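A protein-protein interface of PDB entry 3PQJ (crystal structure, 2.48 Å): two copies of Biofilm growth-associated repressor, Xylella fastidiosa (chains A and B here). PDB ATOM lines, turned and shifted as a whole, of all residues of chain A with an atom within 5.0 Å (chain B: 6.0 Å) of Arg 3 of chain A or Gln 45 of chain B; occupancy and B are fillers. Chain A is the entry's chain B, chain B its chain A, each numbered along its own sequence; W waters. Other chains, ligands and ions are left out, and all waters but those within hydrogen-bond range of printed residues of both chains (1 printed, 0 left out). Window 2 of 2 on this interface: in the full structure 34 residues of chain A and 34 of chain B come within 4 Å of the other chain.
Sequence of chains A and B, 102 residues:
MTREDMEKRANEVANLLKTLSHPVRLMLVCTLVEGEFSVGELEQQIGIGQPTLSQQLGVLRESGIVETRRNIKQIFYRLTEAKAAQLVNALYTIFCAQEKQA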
ATOM      1  N   MET A   1      34.742  11.607 -11.121  1.00  0.00           N
ATOM      2  CA  MET A   1      35.674  10.744 -10.404  1.00  0.00           C
ATOM      3  C   MET A   1      35.070   9.360 -10.134  1.00  0.00           C
ATOM      4  O   MET A   1      35.815   8.416  -9.887  1.00  0.00           O
ATOM      5  CB  MET A   1      36.164  11.428  -9.108  1.00  0.00           C
ATOM      6  CG  MET A   1      37.633  11.151  -8.779  1.00  0.00           C
ATOM      7  SD  MET A   1      38.385  12.294  -7.592  1.00  0.00           S
ATOM      8  CE  MET A   1      38.789  13.648  -8.676  1.00  0.00           C
ATOM      9  N   THR A   2      33.736   9.243 -10.195  1.00  0.00           N
ATOM     10  CA  THR A   2      33.041   7.996  -9.910  1.00  0.00           C
ATOM     11  C   THR A   2      32.736   7.208 -11.182  1.00  0.00           C
ATOM     12  O   THR A   2      32.818   7.746 -12.293  1.00  0.00           O
ATOM     13  CB  THR A   2      31.762   8.255  -9.056  1.00  0.00           C
ATOM     14  OG1 THR A   2      30.799   8.990  -9.815  1.00  0.00           O
ATOM     15  CG2 THR A   2      32.051   8.959  -7.724  1.00  0.00           C
ATOM     16  N   ARG A   3      32.351   5.925 -11.003  1.00  0.00           N
ATOM     17  CA  ARG A   3      31.943   5.036 -12.083  1.00  0.00           C
ATOM     18  C   ARG A   3      30.582   5.485 -12.626  1.00  0.00           C
ATOM     19  O   ARG A   3      30.315   5.306 -13.809  1.00  0.00           O
ATOM     20  CB  ARG A   3      31.949   3.566 -11.624  1.00  0.00           C
ATOM     21  CG  ARG A   3      31.452   2.586 -12.691  1.00  0.00           C
ATOM     22  CD  ARG A   3      32.006   1.192 -12.536  1.00  0.00           C
ATOM     23  NE  ARG A   3      31.803   0.625 -11.199  1.00  0.00           N
ATOM     24  CZ  ARG A   3      30.670   0.092 -10.761  1.00  0.00           C
ATOM     25  NH1 ARG A   3      29.594   0.073 -11.534  1.00  0.00           N
ATOM     26  NH2 ARG A   3      30.599  -0.418  -9.540  1.00  0.00           N
ATOM     27  N   GLU A   4      29.750   6.110 -11.771  1.00  0.00           N
ATOM     28  CA  GLU A   4      28.458   6.673 -12.170  1.00  0.00           C
ATOM     29  C   GLU A   4      28.673   7.831 -13.185  1.00  0.00           C
ATOM     30  O   GLU A   4      28.010   7.831 -14.216  1.00  0.00           O
ATOM     31  CB  GLU A   4      27.625   7.093 -10.943  1.00  0.00           C
ATOM     32  N   ASP A   5      29.646   8.751 -12.945  1.00  0.00           N
ATOM     33  CA  ASP A   5      29.960   9.827 -13.911  1.00  0.00           C
ATOM     34  C   ASP A   5      30.596   9.234 -15.184  1.00  0.00           C
ATOM     35  O   ASP A   5      30.240   9.652 -16.296  1.00  0.00           O
ATOM     36  CB  ASP A   5      30.827  10.974 -13.315  1.00  0.00           C
ATOM     37  CG  ASP A   5      31.167  12.127 -14.290  1.00  0.00           C
ATOM     38  OD1 ASP A   5      30.352  12.397 -15.219  1.00  0.00           O
ATOM     39  OD2 ASP A   5      32.228  12.786 -14.098  1.00  0.00           O
ATOM     40  N   MET A   6      31.496   8.229 -15.012  1.00  0.00           N
ATOM     41  CA  MET A   6      32.118   7.521 -16.140  1.00  0.00           C
ATOM     42  C   MET A   6      31.055   6.894 -17.046  1.00  0.00           C
ATOM     43  O   MET A   6      31.139   7.024 -18.268  1.00  0.00           O
ATOM     44  CB  MET A   6      33.144   6.475 -15.661  1.00  0.00           C
ATOM     45  CG  MET A   6      33.959   5.849 -16.781  1.00  0.00           C
ATOM     46  SD  MET A   6      34.810   6.972 -17.942  1.00  0.00           S
ATOM     47  CE  MET A   6      35.333   5.787 -19.124  1.00  0.00           C
ATOM     48  N   GLU A   7      30.021   6.276 -16.435  1.00  0.00           N
ATOM     49  CA  GLU A   7      28.883   5.650 -17.116  1.00  0.00           C
ATOM     50  C   GLU A   7      28.140   6.677 -17.988  1.00  0.00           C
ATOM     51  O   GLU A   7      27.741   6.345 -19.103  1.00  0.00           O
ATOM     52  CB  GLU A   7      27.936   5.025 -16.082  1.00  0.00           C
ATOM     53  CG  GLU A   7      27.022   3.941 -16.619  1.00  0.00           C
ATOM     54  CD  GLU A   7      26.816   2.791 -15.658  1.00  0.00           C
ATOM     55  OE1 GLU A   7      27.817   2.120 -15.314  1.00  0.00           O
ATOM     56  OE2 GLU A   7      25.661   2.578 -15.222  1.00  0.00           O
ATOM     57  N   MET B  27      31.935  -0.176 -19.989  1.00  0.00           N
ATOM     58  CA  MET B  27      31.312  -0.137 -18.661  1.00  0.00           C
ATOM     59  C   MET B  27      31.607  -1.427 -17.889  1.00  0.00           C
ATOM     60  O   MET B  27      31.823  -1.368 -16.687  1.00  0.00           O
ATOM     61  CB  MET B  27      29.789   0.109 -18.723  1.00  0.00           C
ATOM     62  CG  MET B  27      29.331   1.483 -19.264  1.00  0.00           C
ATOM     63  SD  MET B  27      27.573   1.326 -19.926  1.00  0.00           S
ATOM     64  CE  MET B  27      27.391   2.824 -20.775  1.00  0.00           C
ATOM     65  N   CYS B  30      35.274  -1.156 -16.714  1.00  0.00           N
ATOM     66  CA  CYS B  30      35.301  -0.137 -15.665  1.00  0.00           C
ATOM     67  C   CYS B  30      34.815  -0.722 -14.341  1.00  0.00           C
ATOM     68  O   CYS B  30      35.393  -0.435 -13.303  1.00  0.00           O
ATOM     69  CB  CYS B  30      34.477   1.075 -16.078  1.00  0.00           C
ATOM     70  SG  CYS B  30      35.281   2.115 -17.306  1.00  0.00           S
ATOM     71  N   THR B  31      33.771  -1.562 -14.391  1.00  0.00           N
ATOM     72  CA  THR B  31      33.220  -2.243 -13.221  1.00  0.00           C
ATOM     73  C   THR B  31      34.243  -3.244 -12.692  1.00  0.00           C
ATOM     74  O   THR B  31      34.575  -3.205 -11.509  1.00  0.00           O
ATOM     75  CB  THR B  31      31.882  -2.887 -13.585  1.00  0.00           C
ATOM     76  OG1 THR B  31      31.053  -1.865 -14.133  1.00  0.00           O
ATOM     77  CG2 THR B  31      31.182  -3.543 -12.380  1.00  0.00           C
ATOM     78  N   GLU B  34      37.400  -2.884 -10.084  1.00  0.00           N
ATOM     79  CA  GLU B  34      37.020  -2.834  -8.677  1.00  0.00           C
ATOM     80  C   GLU B  34      37.103  -4.178  -7.971  1.00  0.00           C
ATOM     81  O   GLU B  34      37.274  -4.220  -6.757  1.00  0.00           O
ATOM     82  CB  GLU B  34      35.597  -2.277  -8.546  1.00  0.00           C
ATOM     83  CG  GLU B  34      35.435  -0.857  -9.053  1.00  0.00           C
ATOM     84  CD  GLU B  34      34.013  -0.335  -9.075  1.00  0.00           C
ATOM     85  OE1 GLU B  34      33.117  -0.957  -8.457  1.00  0.00           O
ATOM     86  OE2 GLU B  34      33.800   0.717  -9.716  1.00  0.00           O
ATOM     87  N   PHE B  37      32.943  -9.817 -10.115  1.00  0.00           N
ATOM     88  CA  PHE B  37      31.486  -9.708 -10.097  1.00  0.00           C
ATOM     89  C   PHE B  37      30.870 -10.883 -10.850  1.00  0.00           C
ATOM     90  O   PHE B  37      31.404 -11.309 -11.881  1.00  0.00           O
ATOM     91  CB  PHE B  37      31.019  -8.393 -10.768  1.00  0.00           C
ATOM     92  CG  PHE B  37      31.344  -7.118 -10.031  1.00  0.00           C
ATOM     93  CD1 PHE B  37      30.444  -6.570  -9.124  1.00  0.00           C
ATOM     94  CD2 PHE B  37      32.536  -6.431 -10.280  1.00  0.00           C
ATOM     95  CE1 PHE B  37      30.748  -5.376  -8.445  1.00  0.00           C
ATOM     96  CE2 PHE B  37      32.853  -5.244  -9.588  1.00  0.00           C
ATOM     97  CZ  PHE B  37      31.953  -4.717  -8.685  1.00  0.00           C
ATOM     98  N   GLY B  40      25.034 -11.768 -12.677  1.00  0.00           N
ATOM     99  CA  GLY B  40      23.906 -11.119 -12.011  1.00  0.00           C
ATOM    100  C   GLY B  40      24.272  -9.773 -11.433  1.00  0.00           C
ATOM    101  O   GLY B  40      23.547  -8.810 -11.658  1.00  0.00           O
ATOM    102  N   GLU B  41      25.415  -9.684 -10.718  1.00  0.00           N
ATOM    103  CA  GLU B  41      25.933  -8.427 -10.139  1.00  0.00           C
ATOM    104  C   GLU B  41      26.266  -7.406 -11.246  1.00  0.00           C
ATOM    105  O   GLU B  41      26.035  -6.218 -11.052  1.00  0.00           O
ATOM    106  CB  GLU B  41      27.209  -8.683  -9.330  1.00  0.00           C
ATOM    107  CG  GLU B  41      27.017  -9.305  -7.962  1.00  0.00           C
ATOM    108  CD  GLU B  41      28.335  -9.556  -7.257  1.00  0.00           C
ATOM    109  OE1 GLU B  41      28.894 -10.660  -7.435  1.00  0.00           O
ATOM    110  OE2 GLU B  41      28.846  -8.626  -6.592  1.00  0.00           O
ATOM    111  N   LEU B  42      26.819  -7.873 -12.394  1.00  0.00           N
ATOM    112  CA  LEU B  42      27.174  -7.032 -13.544  1.00  0.00           C
ATOM    113  C   LEU B  42      25.944  -6.431 -14.214  1.00  0.00           C
ATOM    114  O   LEU B  42      26.003  -5.306 -14.710  1.00  0.00           O
ATOM    115  CB  LEU B  42      28.031  -7.799 -14.576  1.00  0.00           C
ATOM    116  CG  LEU B  42      29.497  -8.030 -14.208  1.00  0.00           C
ATOM    117  CD1 LEU B  42      30.128  -9.063 -15.130  1.00  0.00           C
ATOM    118  CD2 LEU B  42      30.286  -6.715 -14.202  1.00  0.00           C
ATOM    119  N   GLU B  43      24.832  -7.190 -14.222  1.00  0.00           N
ATOM    120  CA  GLU B  43      23.536  -6.780 -14.757  1.00  0.00           C
ATOM    121  C   GLU B  43      23.007  -5.635 -13.888  1.00  0.00           C
ATOM    122  O   GLU B  43      22.502  -4.647 -14.419  1.00  0.00           O
ATOM    123  CB  GLU B  43      22.589  -7.985 -14.749  1.00  0.00           C
ATOM    124  CG  GLU B  43      21.232  -7.760 -15.403  1.00  0.00           C
ATOM    125  CD  GLU B  43      20.408  -9.012 -15.643  1.00  0.00           C
ATOM    126  OE1 GLU B  43      20.664 -10.041 -14.971  1.00  0.00           O
ATOM    127  OE2 GLU B  43      19.490  -8.956 -16.494  1.00  0.00           O
ATOM    128  N   GLN B  44      23.194  -5.747 -12.560  1.00  0.00           N
ATOM    129  CA  GLN B  44      22.780  -4.741 -11.579  1.00  0.00           C
ATOM    130  C   GLN B  44      23.659  -3.499 -11.669  1.00  0.00           C
ATOM    131  O   GLN B  44      23.150  -2.383 -11.532  1.00  0.00           O
ATOM    132  CB  GLN B  44      22.783  -5.301 -10.134  1.00  0.00           C
ATOM    133  CG  GLN B  44      22.007  -6.620  -9.870  1.00  0.00           C
ATOM    134  CD  GLN B  44      20.681  -6.835 -10.602  1.00  0.00           C
ATOM    135  OE1 GLN B  44      19.933  -5.888 -10.902  1.00  0.00           O
ATOM    136  NE2 GLN B  44      20.324  -8.100 -10.844  1.00  0.00           N
ATOM    137  N   GLN B  45      24.970  -3.691 -11.913  1.00  0.00           N
ATOM    138  CA  GLN B  45      25.929  -2.601 -12.001  1.00  0.00           C
ATOM    139  C   GLN B  45      25.821  -1.737 -13.253  1.00  0.00           C
ATOM    140  O   GLN B  45      25.878  -0.516 -13.133  1.00  0.00           O
ATOM    141  CB  GLN B  45      27.368  -3.104 -11.797  1.00  0.00           C
ATOM    142  CG  GLN B  45      27.726  -3.499 -10.350  1.00  0.00           C
ATOM    143  CD  GLN B  45      27.399  -2.462  -9.301  1.00  0.00           C
ATOM    144  OE1 GLN B  45      27.751  -1.275  -9.392  1.00  0.00           O
ATOM    145  NE2 GLN B  45      26.746  -2.921  -8.258  1.00  0.00           N
ATOM    146  N   ILE B  46      25.688  -2.340 -14.440  1.00  0.00           N
ATOM    147  CA  ILE B  46      25.652  -1.582 -15.685  1.00  0.00           C
ATOM    148  C   ILE B  46      24.253  -1.318 -16.266  1.00  0.00           C
ATOM    149  O   ILE B  46      24.118  -0.443 -17.114  1.00  0.00           O
ATOM    150  CB  ILE B  46      26.740  -2.026 -16.714  1.00  0.00           C
ATOM    151  CG1 ILE B  46      26.350  -3.297 -17.491  1.00  0.00           C
ATOM    152  CG2 ILE B  46      28.126  -2.171 -16.045  1.00  0.00           C
ATOM    153  CD1 ILE B  46      26.981  -3.396 -18.945  1.00  0.00           C
ATOM    154  N   GLY B  47      23.232  -2.023 -15.764  1.00  0.00           N
ATOM    155  CA  GLY B  47      21.844  -1.864 -16.206  1.00  0.00           C
ATOM    156  C   GLY B  47      21.557  -2.321 -17.627  1.00  0.00           C
ATOM    157  O   GLY B  47      20.827  -1.661 -18.376  1.00  0.00           O
ATOM    158  N   TYR B  92      39.784   7.791 -16.518  1.00  0.00           N
ATOM    159  CA  TYR B  92      39.217   8.557 -15.389  1.00  0.00           C
ATOM    160  C   TYR B  92      39.887   9.926 -15.291  1.00  0.00           C
ATOM    161  O   TYR B  92      39.204  10.940 -15.223  1.00  0.00           O
ATOM    162  CB  TYR B  92      39.346   7.790 -14.057  1.00  0.00           C
ATOM    163  CG  TYR B  92      38.203   6.811 -13.824  1.00  0.00           C
ATOM    164  CD1 TYR B  92      37.054   7.192 -13.127  1.00  0.00           C
ATOM    165  CD2 TYR B  92      38.257   5.518 -14.331  1.00  0.00           C
ATOM    166  CE1 TYR B  92      35.982   6.307 -12.954  1.00  0.00           C
ATOM    167  CE2 TYR B  92      37.195   4.628 -14.170  1.00  0.00           C
ATOM    168  CZ  TYR B  92      36.060   5.024 -13.477  1.00  0.00           C
ATOM    169  OH  TYR B  92      35.022   4.133 -13.332  1.00  0.00           O
HETATM  170  O   HOH W   1      28.024   0.862 -13.237  1.00  0.00           O
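The guanidinium group (NE) of Arg 3 of chain A is in salt-bridge range of the side-chain carboxylate (OE2) of Glu 34 of chain B, 2.5 Å away. The side-chain amide oxygen (OE1) of Gln 45 of chain B is in hydrogen-bond range of the guanidinium group (NH2) of Arg 3 of chain A (3.0 Å).
The side-chain hydroxyl (OG1) of Thr 31 of chain B sits at hydrogen-bond distance from the backbone carbonyl oxygen (O) of Met 27 of chain B, 2.7 Å away. OG1 of Thr 2 of chain A lies within hydrogen-bond range of N of Asp 5 of chain A, 3.3 Å away.
O of Met 1 of chain A touches CD1 of Tyr 92 of chain B (3.7 Å). Thr 2 of chain A touches Tyr 92 of chain B. Arg 3 of chain A touches Cys 30 of chain B. Arg 3 of chain A touches Thr 31 of chain B. Arg 3 of chain A touches Tyr 92 of chain B (CA to OH, 3.4 Å). Cys 30 of chain B touches Met 6 of chain A. OH of Tyr 92 of chain B touches CB of Met 6 of chain A, 3.8 Å away. Met 27 of chain B touches Glu 7 of chain A (CE to O, 3.9 Å). OE2 of Glu 7 of chain A touches O of Gln 45 of chain B, 3.7 Å away. Glu 7 of chain A touches Ile 46 of chain B (OE2 to O, 3.9 Å).
Of chain B, only Cys 30 (3.8 Å), Thr 31 (3.6 Å), Glu 34 (2.5 Å), Gln 45 (3.0 Å) and Tyr 92 (3.4 Å) come within 4 Å of Arg 3 of chain A. Gln 45 of chain B touches two residues of chain A. Of the printed residues of chain A, Met 27 of chain B touches Glu 7 (3.9 Å). Of the printed residues of chain B, Thr 2 of chain A touches Tyr 92 (3.5 Å). Of the printed residues of chain B, Glu 7 of chain A touches Met 27, Gln 45 and Ile 46. Of the printed residues of chain A, Tyr 92 of chain B touches Met 1, Thr 2, Arg 3 and Met 6. Printed residues of chain A within 4 Å of Ile 46 of chain B: Glu 7. Asp 5 of chain A touches none of the printed residues of chain B. The nearest residue of chain B that does not touch Arg 3 of chain A is Phe 37 of chain B (4.6 Å).
Hydrophobic or aromatic side chains of chain A that line the printed part of chain B: Met 6. Among the printed residues, 12 pairs touch across the chains. Among the printed residues, Asp or Glu carboxylates within 4 Å of a Lys or Arg side-chain nitrogen of the other chain: Arg 3 of chain A with Glu 34 of chain B (2.5 Å).
No position is printed for both chains. Of the 12 pairs that touch across the chains among the printed residues, none has its exchanged pair printed and touching as well.
Water W1 lies within hydrogen-bond range of the side-chain carboxylate (OE1) of Glu 7 of chain A (2.4 Å), the guanidinium group (NH1) of Arg 3 of chain A (2.4 Å) and the backbone carbonyl oxygen (O) of Gln 45 of chain B (2.6 Å).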
